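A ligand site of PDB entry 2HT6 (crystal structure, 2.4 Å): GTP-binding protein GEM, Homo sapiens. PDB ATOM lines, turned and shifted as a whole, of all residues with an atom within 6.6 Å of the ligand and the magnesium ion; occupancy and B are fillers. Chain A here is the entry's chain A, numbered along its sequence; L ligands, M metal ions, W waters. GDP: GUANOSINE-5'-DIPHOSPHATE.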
ATOM      1  N   GLY A  13      32.114  14.582 -14.944  1.00  0.00           N
ATOM      2  CA  GLY A  13      31.154  15.652 -14.843  1.00  0.00           C
ATOM      3  C   GLY A  13      31.672  16.759 -13.956  1.00  0.00           C
ATOM      4  O   GLY A  13      32.614  16.568 -13.193  1.00  0.00           O
ATOM      5  N   GLU A  14      31.036  17.922 -14.078  1.00  0.00           N
ATOM      6  CA  GLU A  14      31.309  19.092 -13.234  1.00  0.00           C
ATOM      7  C   GLU A  14      31.221  18.782 -11.727  1.00  0.00           C
ATOM      8  O   GLU A  14      30.608  17.807 -11.340  1.00  0.00           O
ATOM      9  CB  GLU A  14      30.352  20.223 -13.622  1.00  0.00           C
ATOM     10  CG  GLU A  14      30.796  21.637 -13.225  1.00  0.00           C
ATOM     11  CD  GLU A  14      32.180  21.981 -13.757  1.00  0.00           C
ATOM     12  OE1 GLU A  14      32.360  22.068 -14.989  1.00  0.00           O
ATOM     13  OE2 GLU A  14      33.112  22.166 -12.935  1.00  0.00           O
ATOM     14  N   GLN A  15      31.855  19.610 -10.915  1.00  0.00           N
ATOM     15  CA  GLN A  15      31.840  19.496  -9.451  1.00  0.00           C
ATOM     16  C   GLN A  15      30.442  19.648  -8.899  1.00  0.00           C
ATOM     17  O   GLN A  15      29.659  20.463  -9.383  1.00  0.00           O
ATOM     18  CB  GLN A  15      32.743  20.580  -8.836  1.00  0.00           C
ATOM     19  CG  GLN A  15      32.988  20.473  -7.314  1.00  0.00           C
ATOM     20  CD  GLN A  15      34.229  19.669  -6.919  1.00  0.00           C
ATOM     21  OE1 GLN A  15      34.561  19.576  -5.728  1.00  0.00           O
ATOM     22  NE2 GLN A  15      34.921  19.076  -7.898  1.00  0.00           N
ATOM     23  N   GLY A  16      30.131  18.845  -7.879  1.00  0.00           N
ATOM     24  CA  GLY A  16      28.844  18.884  -7.174  1.00  0.00           C
ATOM     25  C   GLY A  16      27.636  18.284  -7.859  1.00  0.00           C
ATOM     26  O   GLY A  16      26.514  18.391  -7.334  1.00  0.00           O
ATOM     27  N   VAL A  17      27.826  17.653  -9.030  1.00  0.00           N
ATOM     28  CA  VAL A  17      26.701  17.057  -9.785  1.00  0.00           C
ATOM     29  C   VAL A  17      26.134  15.761  -9.145  1.00  0.00           C
ATOM     30  O   VAL A  17      24.986  15.389  -9.389  1.00  0.00           O
ATOM     31  CB  VAL A  17      27.035  16.865 -11.302  1.00  0.00           C
ATOM     32  CG1 VAL A  17      27.490  18.190 -11.924  1.00  0.00           C
ATOM     33  CG2 VAL A  17      28.084  15.786 -11.521  1.00  0.00           C
ATOM     34  N   GLY A  18      26.942  15.081  -8.324  1.00  0.00           N
ATOM     35  CA  GLY A  18      26.496  13.861  -7.637  1.00  0.00           C
ATOM     36  C   GLY A  18      27.300  12.599  -7.948  1.00  0.00           C
ATOM     37  O   GLY A  18      26.842  11.478  -7.669  1.00  0.00           O
ATOM     38  N   LYS A  19      28.497  12.752  -8.502  1.00  0.00           N
ATOM     39  CA  LYS A  19      29.286  11.590  -8.881  1.00  0.00           C
ATOM     40  C   LYS A  19      29.614  10.683  -7.678  1.00  0.00           C
ATOM     41  O   LYS A  19      29.351   9.464  -7.706  1.00  0.00           O
ATOM     42  CB  LYS A  19      30.555  12.026  -9.617  1.00  0.00           C
ATOM     43  CG  LYS A  19      30.305  12.930 -10.828  1.00  0.00           C
ATOM     44  CD  LYS A  19      31.567  13.183 -11.683  1.00  0.00           C
ATOM     45  CE  LYS A  19      32.625  14.021 -10.959  1.00  0.00           C
ATOM     46  NZ  LYS A  19      32.061  15.309 -10.453  1.00  0.00           N
ATOM     47  N   SER A  20      30.172  11.284  -6.632  1.00  0.00           N
ATOM     48  CA  SER A  20      30.538  10.539  -5.418  1.00  0.00           C
ATOM     49  C   SER A  20      29.327   9.923  -4.722  1.00  0.00           C
ATOM     50  O   SER A  20      29.428   8.807  -4.213  1.00  0.00           O
ATOM     51  CB  SER A  20      31.339  11.425  -4.464  1.00  0.00           C
ATOM     52  OG  SER A  20      32.430  12.017  -5.140  1.00  0.00           O
ATOM     53  N   THR A  21      28.203  10.636  -4.725  1.00  0.00           N
ATOM     54  CA  THR A  21      26.978  10.090  -4.163  1.00  0.00           C
ATOM     55  C   THR A  21      26.494   8.882  -4.975  1.00  0.00           C
ATOM     56  O   THR A  21      26.035   7.896  -4.378  1.00  0.00           O
ATOM     57  CB  THR A  21      25.865  11.134  -4.041  1.00  0.00           C
ATOM     58  OG1 THR A  21      26.405  12.343  -3.481  1.00  0.00           O
ATOM     59  CG2 THR A  21      24.766  10.610  -3.133  1.00  0.00           C
ATOM     60  N   LEU A  22      26.570   8.957  -6.305  1.00  0.00           N
ATOM     61  CA  LEU A  22      26.251   7.806  -7.162  1.00  0.00           C
ATOM     62  C   LEU A  22      27.166   6.634  -6.872  1.00  0.00           C
ATOM     63  O   LEU A  22      26.690   5.497  -6.720  1.00  0.00           O
ATOM     64  CB  LEU A  22      26.295   8.169  -8.652  1.00  0.00           C
ATOM     65  CG  LEU A  22      25.143   9.081  -9.132  1.00  0.00           C
ATOM     66  CD1 LEU A  22      25.470   9.764 -10.448  1.00  0.00           C
ATOM     67  CD2 LEU A  22      23.798   8.331  -9.209  1.00  0.00           C
ATOM     68  N   ASN A  24      28.929   5.857  -4.217  1.00  0.00           N
ATOM     69  CA  ASN A  24      28.686   5.304  -2.882  1.00  0.00           C
ATOM     70  C   ASN A  24      27.486   4.376  -2.831  1.00  0.00           C
ATOM     71  O   ASN A  24      27.551   3.330  -2.182  1.00  0.00           O
ATOM     72  CB  ASN A  24      28.499   6.442  -1.868  1.00  0.00           C
ATOM     73  CG  ASN A  24      29.779   7.228  -1.643  1.00  0.00           C
ATOM     74  OD1 ASN A  24      30.889   6.676  -1.694  1.00  0.00           O
ATOM     75  ND2 ASN A  24      29.631   8.547  -1.391  1.00  0.00           N
ATOM     76  N   ASP A  62      35.826   7.094  -9.667  1.00  0.00           N
ATOM     77  CA  ASP A  62      35.247   8.375  -9.291  1.00  0.00           C
ATOM     78  C   ASP A  62      36.378   9.327  -8.885  1.00  0.00           C
ATOM     79  O   ASP A  62      36.419   9.801  -7.744  1.00  0.00           O
ATOM     80  CB  ASP A  62      34.221   8.194  -8.162  1.00  0.00           C
ATOM     81  CG  ASP A  62      33.687   9.526  -7.610  1.00  0.00           C
ATOM     82  OD1 ASP A  62      33.474   9.604  -6.382  1.00  0.00           O
ATOM     83  OD2 ASP A  62      33.480  10.488  -8.391  1.00  0.00           O
ATOM     84  N   TRP A  64      37.379  12.104 -10.928  1.00  0.00           N
ATOM     85  CA  TRP A  64      37.316  13.297 -11.758  1.00  0.00           C
ATOM     86  C   TRP A  64      37.013  14.529 -10.889  1.00  0.00           C
ATOM     87  O   TRP A  64      35.927  14.657 -10.340  1.00  0.00           O
ATOM     88  CB  TRP A  64      36.290  13.106 -12.866  1.00  0.00           C
ATOM     89  CG  TRP A  64      36.308  14.160 -13.915  1.00  0.00           C
ATOM     90  CD1 TRP A  64      35.645  15.355 -13.875  1.00  0.00           C
ATOM     91  CD2 TRP A  64      36.973  14.114 -15.186  1.00  0.00           C
ATOM     92  NE1 TRP A  64      35.866  16.060 -15.026  1.00  0.00           N
ATOM     93  CE2 TRP A  64      36.684  15.331 -15.845  1.00  0.00           C
ATOM     94  CE3 TRP A  64      37.780  13.176 -15.818  1.00  0.00           C
ATOM     95  CZ2 TRP A  64      37.199  15.629 -17.122  1.00  0.00           C
ATOM     96  CZ3 TRP A  64      38.292  13.464 -17.091  1.00  0.00           C
ATOM     97  CH2 TRP A  64      37.994  14.682 -17.729  1.00  0.00           C
ATOM     98  N   GLU A  65      38.008  15.412 -10.762  1.00  0.00           N
ATOM     99  CA  GLU A  65      37.852  16.675 -10.038  1.00  0.00           C
ATOM    100  C   GLU A  65      38.099  17.833 -11.006  1.00  0.00           C
ATOM    101  O   GLU A  65      38.547  17.618 -12.132  1.00  0.00           O
ATOM    102  CB  GLU A  65      38.821  16.787  -8.836  1.00  0.00           C
ATOM    103  CG  GLU A  65      38.823  15.599  -7.877  1.00  0.00           C
ATOM    104  CD  GLU A  65      37.546  15.484  -7.052  1.00  0.00           C
ATOM    105  OE1 GLU A  65      36.604  14.770  -7.485  1.00  0.00           O
ATOM    106  OE2 GLU A  65      37.483  16.102  -5.961  1.00  0.00           O
ATOM    107  N   VAL A  87      27.815  12.893 -16.037  1.00  0.00           N
ATOM    108  CA  VAL A  87      26.793  13.318 -15.092  1.00  0.00           C
ATOM    109  C   VAL A  87      26.689  14.835 -15.058  1.00  0.00           C
ATOM    110  O   VAL A  87      27.693  15.549 -15.004  1.00  0.00           O
ATOM    111  CB  VAL A  87      27.121  12.775 -13.667  1.00  0.00           C
ATOM    112  CG1 VAL A  87      25.970  13.023 -12.696  1.00  0.00           C
ATOM    113  CG2 VAL A  87      27.443  11.274 -13.731  1.00  0.00           C
ATOM    114  N   ASN A 122      21.331  14.071 -12.977  1.00  0.00           N
ATOM    115  CA  ASN A 122      21.113  13.764 -11.550  1.00  0.00           C
ATOM    116  C   ASN A 122      20.305  14.860 -10.813  1.00  0.00           C
ATOM    117  O   ASN A 122      20.090  15.956 -11.337  1.00  0.00           O
ATOM    118  CB  ASN A 122      22.455  13.481 -10.841  1.00  0.00           C
ATOM    119  CG  ASN A 122      22.291  12.938  -9.403  1.00  0.00           C
ATOM    120  OD1 ASN A 122      21.513  12.017  -9.157  1.00  0.00           O
ATOM    121  ND2 ASN A 122      23.046  13.510  -8.453  1.00  0.00           N
ATOM    122  N   LYS A 123      19.837  14.529  -9.608  1.00  0.00           N
ATOM    123  CA  LYS A 123      19.118  15.456  -8.707  1.00  0.00           C
ATOM    124  C   LYS A 123      17.657  15.708  -9.121  1.00  0.00           C
ATOM    125  O   LYS A 123      17.126  16.797  -8.924  1.00  0.00           O
ATOM    126  CB  LYS A 123      19.869  16.785  -8.540  1.00  0.00           C
ATOM    127  CG  LYS A 123      21.308  16.606  -8.101  1.00  0.00           C
ATOM    128  CD  LYS A 123      21.852  17.873  -7.453  1.00  0.00           C
ATOM    129  CE  LYS A 123      23.295  17.689  -6.998  1.00  0.00           C
ATOM    130  NZ  LYS A 123      23.947  19.026  -6.798  1.00  0.00           N
ATOM    131  N   SER A 124      17.023  14.680  -9.689  1.00  0.00           N
ATOM    132  CA  SER A 124      15.631  14.788 -10.157  1.00  0.00           C
ATOM    133  C   SER A 124      14.609  15.025  -9.021  1.00  0.00           C
ATOM    134  O   SER A 124      13.488  15.483  -9.277  1.00  0.00           O
ATOM    135  CB  SER A 124      15.230  13.582 -11.014  1.00  0.00           C
ATOM    136  OG  SER A 124      15.376  12.363 -10.295  1.00  0.00           O
ATOM    137  N   ASP A 125      15.019  14.751  -7.780  1.00  0.00           N
ATOM    138  CA  ASP A 125      14.183  15.053  -6.603  1.00  0.00           C
ATOM    139  C   ASP A 125      13.979  16.558  -6.373  1.00  0.00           C
ATOM    140  O   ASP A 125      12.971  16.967  -5.827  1.00  0.00           O
ATOM    141  CB  ASP A 125      14.730  14.368  -5.338  1.00  0.00           C
ATOM    142  CG  ASP A 125      16.152  14.763  -5.015  1.00  0.00           C
ATOM    143  OD1 ASP A 125      17.085  14.426  -5.788  1.00  0.00           O
ATOM    144  OD2 ASP A 125      16.348  15.387  -3.948  1.00  0.00           O
ATOM    145  N   LEU A 126      14.934  17.375  -6.824  1.00  0.00           N
ATOM    146  CA  LEU A 126      14.885  18.822  -6.677  1.00  0.00           C
ATOM    147  C   LEU A 126      13.978  19.454  -7.728  1.00  0.00           C
ATOM    148  O   LEU A 126      14.421  20.280  -8.553  1.00  0.00           O
ATOM    149  CB  LEU A 126      16.298  19.391  -6.718  1.00  0.00           C
ATOM    150  CG  LEU A 126      17.019  19.585  -5.383  1.00  0.00           C
ATOM    151  CD1 LEU A 126      16.445  18.811  -4.182  1.00  0.00           C
ATOM    152  CD2 LEU A 126      18.495  19.298  -5.568  1.00  0.00           C
ATOM    153  N   THR A 151      18.418  10.468 -12.756  1.00  0.00           N
ATOM    154  CA  THR A 151      18.524   9.796 -11.467  1.00  0.00           C
ATOM    155  C   THR A 151      18.291  10.775 -10.327  1.00  0.00           C
ATOM    156  O   THR A 151      18.284  12.012 -10.515  1.00  0.00           O
ATOM    157  CB  THR A 151      19.952   9.155 -11.249  1.00  0.00           C
ATOM    158  OG1 THR A 151      20.967  10.168 -11.382  1.00  0.00           O
ATOM    159  CG2 THR A 151      20.240   8.019 -12.218  1.00  0.00           C
ATOM    160  N   SER A 152      18.096  10.211  -9.146  1.00  0.00           N
ATOM    161  CA  SER A 152      18.279  10.960  -7.924  1.00  0.00           C
ATOM    162  C   SER A 152      19.115  10.112  -7.007  1.00  0.00           C
ATOM    163  O   SER A 152      18.625   9.121  -6.442  1.00  0.00           O
ATOM    164  CB  SER A 152      16.939  11.308  -7.268  1.00  0.00           C
ATOM    165  OG  SER A 152      17.195  11.845  -5.994  1.00  0.00           O
ATOM    166  N   ALA A 153      20.388  10.459  -6.896  1.00  0.00           N
ATOM    167  CA  ALA A 153      21.282   9.728  -6.033  1.00  0.00           C
ATOM    168  C   ALA A 153      20.935   9.900  -4.545  1.00  0.00           C
ATOM    169  O   ALA A 153      21.239   9.034  -3.736  1.00  0.00           O
ATOM    170  CB  ALA A 153      22.727  10.140  -6.287  1.00  0.00           C
ATOM    171  N   ALA A 154      20.298  11.025  -4.178  1.00  0.00           N
ATOM    172  CA  ALA A 154      19.927  11.256  -2.777  1.00  0.00           C
ATOM    173  C   ALA A 154      18.937  10.199  -2.307  1.00  0.00           C
ATOM    174  O   ALA A 154      19.115   9.632  -1.224  1.00  0.00           O
ATOM    175  CB  ALA A 154      19.348  12.662  -2.583  1.00  0.00           C
ATOM    176  N   VAL A 155      17.937   9.899  -3.127  1.00  0.00           N
ATOM    177  CA  VAL A 155      16.905   8.915  -2.779  1.00  0.00           C
ATOM    178  C   VAL A 155      17.079   7.536  -3.472  1.00  0.00           C
ATOM    179  O   VAL A 155      16.235   6.648  -3.324  1.00  0.00           O
ATOM    180  CB  VAL A 155      15.505   9.475  -3.063  1.00  0.00           C
ATOM    181  CG1 VAL A 155      14.450   8.545  -2.470  1.00  0.00           C
ATOM    182  CG2 VAL A 155      15.370  10.872  -2.460  1.00  0.00           C
HETATM  183  PB  GDP L   1      30.435  15.340  -7.012  1.00  0.00           P
HETATM  184  O1B GDP L   1      30.023  15.086  -8.437  1.00  0.00           O
HETATM  185  O2B GDP L   1      31.363  16.525  -7.064  1.00  0.00           O
HETATM  186  O3B GDP L   1      31.114  14.146  -6.377  1.00  0.00           O
HETATM  187  O3A GDP L   1      29.092  15.669  -6.217  1.00  0.00           O
HETATM  188  PA  GDP L   1      28.740  15.065  -4.785  1.00  0.00           P
HETATM  189  O1A GDP L   1      29.922  15.297  -3.870  1.00  0.00           O
HETATM  190  O2A GDP L   1      28.311  13.623  -4.869  1.00  0.00           O
HETATM  191  O5' GDP L   1      27.445  15.904  -4.369  1.00  0.00           O
HETATM  192  C5' GDP L   1      27.544  17.240  -3.833  1.00  0.00           C
HETATM  193  C4' GDP L   1      26.284  17.496  -3.021  1.00  0.00           C
HETATM  194  O4' GDP L   1      25.123  17.222  -3.837  1.00  0.00           O
HETATM  195  C3' GDP L   1      26.230  16.565  -1.814  1.00  0.00           C
HETATM  196  O3' GDP L   1      25.953  17.341  -0.653  1.00  0.00           O
HETATM  197  C2' GDP L   1      25.092  15.600  -2.098  1.00  0.00           C
HETATM  198  O2' GDP L   1      24.280  15.404  -0.913  1.00  0.00           O
HETATM  199  C1' GDP L   1      24.233  16.351  -3.125  1.00  0.00           C
HETATM  200  N9  GDP L   1      23.535  15.426  -4.049  1.00  0.00           N
HETATM  201  C8  GDP L   1      24.101  14.478  -4.814  1.00  0.00           C
HETATM  202  N7  GDP L   1      23.172  13.816  -5.540  1.00  0.00           N
HETATM  203  C5  GDP L   1      21.973  14.353  -5.240  1.00  0.00           C
HETATM  204  C6  GDP L   1      20.569  14.122  -5.642  1.00  0.00           C
HETATM  205  O6  GDP L   1      20.292  13.240  -6.473  1.00  0.00           O
HETATM  206  N1  GDP L   1      19.613  14.899  -5.094  1.00  0.00           N
HETATM  207  C2  GDP L   1      19.909  15.856  -4.179  1.00  0.00           C
HETATM  208  N2  GDP L   1      18.908  16.612  -3.657  1.00  0.00           N
HETATM  209  N3  GDP L   1      21.170  16.111  -3.765  1.00  0.00           N
HETATM  210  C4  GDP L   1      22.228  15.411  -4.250  1.00  0.00           C
HETATM  211 MG    MG M   1      33.088  13.841  -5.825  1.00  0.00          MG
HETATM  212  O   HOH W   1      32.354  14.482  -3.758  1.00  0.00           O
HETATM  213  O   HOH W   2      34.894  13.411  -4.911  1.00  0.00           O
HETATM  214  O   HOH W   3      19.095  18.262  -1.294  1.00  0.00           O
HETATM  215  O   HOH W   4      33.784  13.092  -7.801  1.00  0.00           O
HETATM  216  O   HOH W   5      33.670  15.745  -6.295  1.00  0.00           O
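An oxygen (O2A) of the ligand lies within hydrogen-bond range of the backbone NH (N) of Ser 20.
The side-chain carboxylate of Asp 125 lies within hydrogen-bond range of a nitrogen (N1) of the ligand, at 2.7 Å.
The backbone NH (N) of Thr 21 lies within hydrogen-bond range of an oxygen (O2A) of the ligand, at 3.0 Å.
OG1 of Thr 21 is in hydrogen-bond range of O2A of the ligand (2.7 Å).
N of Gly 16 lies within hydrogen-bond range of O2B of the ligand, 2.8 Å away.
N of Lys 19 is in hydrogen-bond range of O1B of the ligand.
O1B of the ligand lies within salt-bridge range of NZ of Lys 19.
N of Ala 153 sits at hydrogen-bond distance from O6 of the ligand, 2.8 Å away.
N7 of the ligand is in hydrogen-bond range of ND2 of Asn 122, at 2.9 Å.
An oxygen (O3A) of the ligand is in hydrogen-bond range of the backbone NH (N) of Gly 18, at 3.1 Å.
O6 of the ligand is in hydrogen-bond range of N of Ala 154, at 3.2 Å.
N of Lys 123 sits close to O6 of the ligand (3.4 Å).
The side-chain hydroxyl of Ser 152 sits close to an oxygen (O6) of the ligand.
The backbone NH (N) of Val 17 sits at hydrogen-bond distance from an oxygen (O1B) of the ligand.
OG of Ser 20 sits close to OD1 of Asp 62.
The side-chain amide nitrogen (ND2) of Asn 24 lies within hydrogen-bond range of the backbone carbonyl oxygen (O) of Ser 20 (2.8 Å).
OG of Ser 152 is in hydrogen-bond range of OD1 of Asp 125, at 2.6 Å.
The backbone carbonyl oxygen (O) of Glu 14 sits at hydrogen-bond distance from the side-chain amino group (NZ) of Lys 19 (3.0 Å).
NZ of Lys 19 is in hydrogen-bond range of O of Gly 13, 3.1 Å away.
OD1 of Asn 122 sits at hydrogen-bond distance from N of Ala 153 (3.0 Å).
OG1 of Thr 151 is in hydrogen-bond range of OD1 of Asn 122 (2.9 Å).
The backbone NH (N) of Lys 123 lies within hydrogen-bond range of the backbone carbonyl oxygen (O) of Thr 151, at 3.1 Å.
Merely in contact with the ligand: Leu 126 (3.3 Å) and Gln 15 (3.7 Å).
Hydrophobic or aromatic side chains within 4 Å of the ligand: Val 17, Leu 126, Ala 153 and Ala 154.
Within 4 Å of the ligand: Gln 15, Gly 16, Val 17, Gly 18, Lys 19, Ser 20, Thr 21, Asn 122, Lys 123, Asp 125, Leu 126, Ser 152, Ala 153 and Ala 154.
The nearest printed residue that does not touch the ligand is Glu 14 (4.02 Å).
Glu 65 touches the magnesium ion (OE1 to MG, 3.998 Å).
Of the 25 residues printed, 2 come within 4 Å of the magnesium ion.
The nearest printed residue that does not touch the magnesium ion is Asp 62 (4.2 Å).
The magnesium ion is bound by water W5 (2.0 Å), OG of Ser 20 (2.1 Å), water W2 (2.1 Å), O3B of the ligand (2.1 Å), water W4 (2.2 Å) and water W1 (2.3 Å).
Water W5 lies within hydrogen-bond range of an oxygen (O2B) of the ligand and the side-chain carboxylate of Glu 65.
Water W4 bridges the side-chain carboxylate (OD2) of Asp 62 and the side-chain carboxylate (OE1) of Glu 65.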
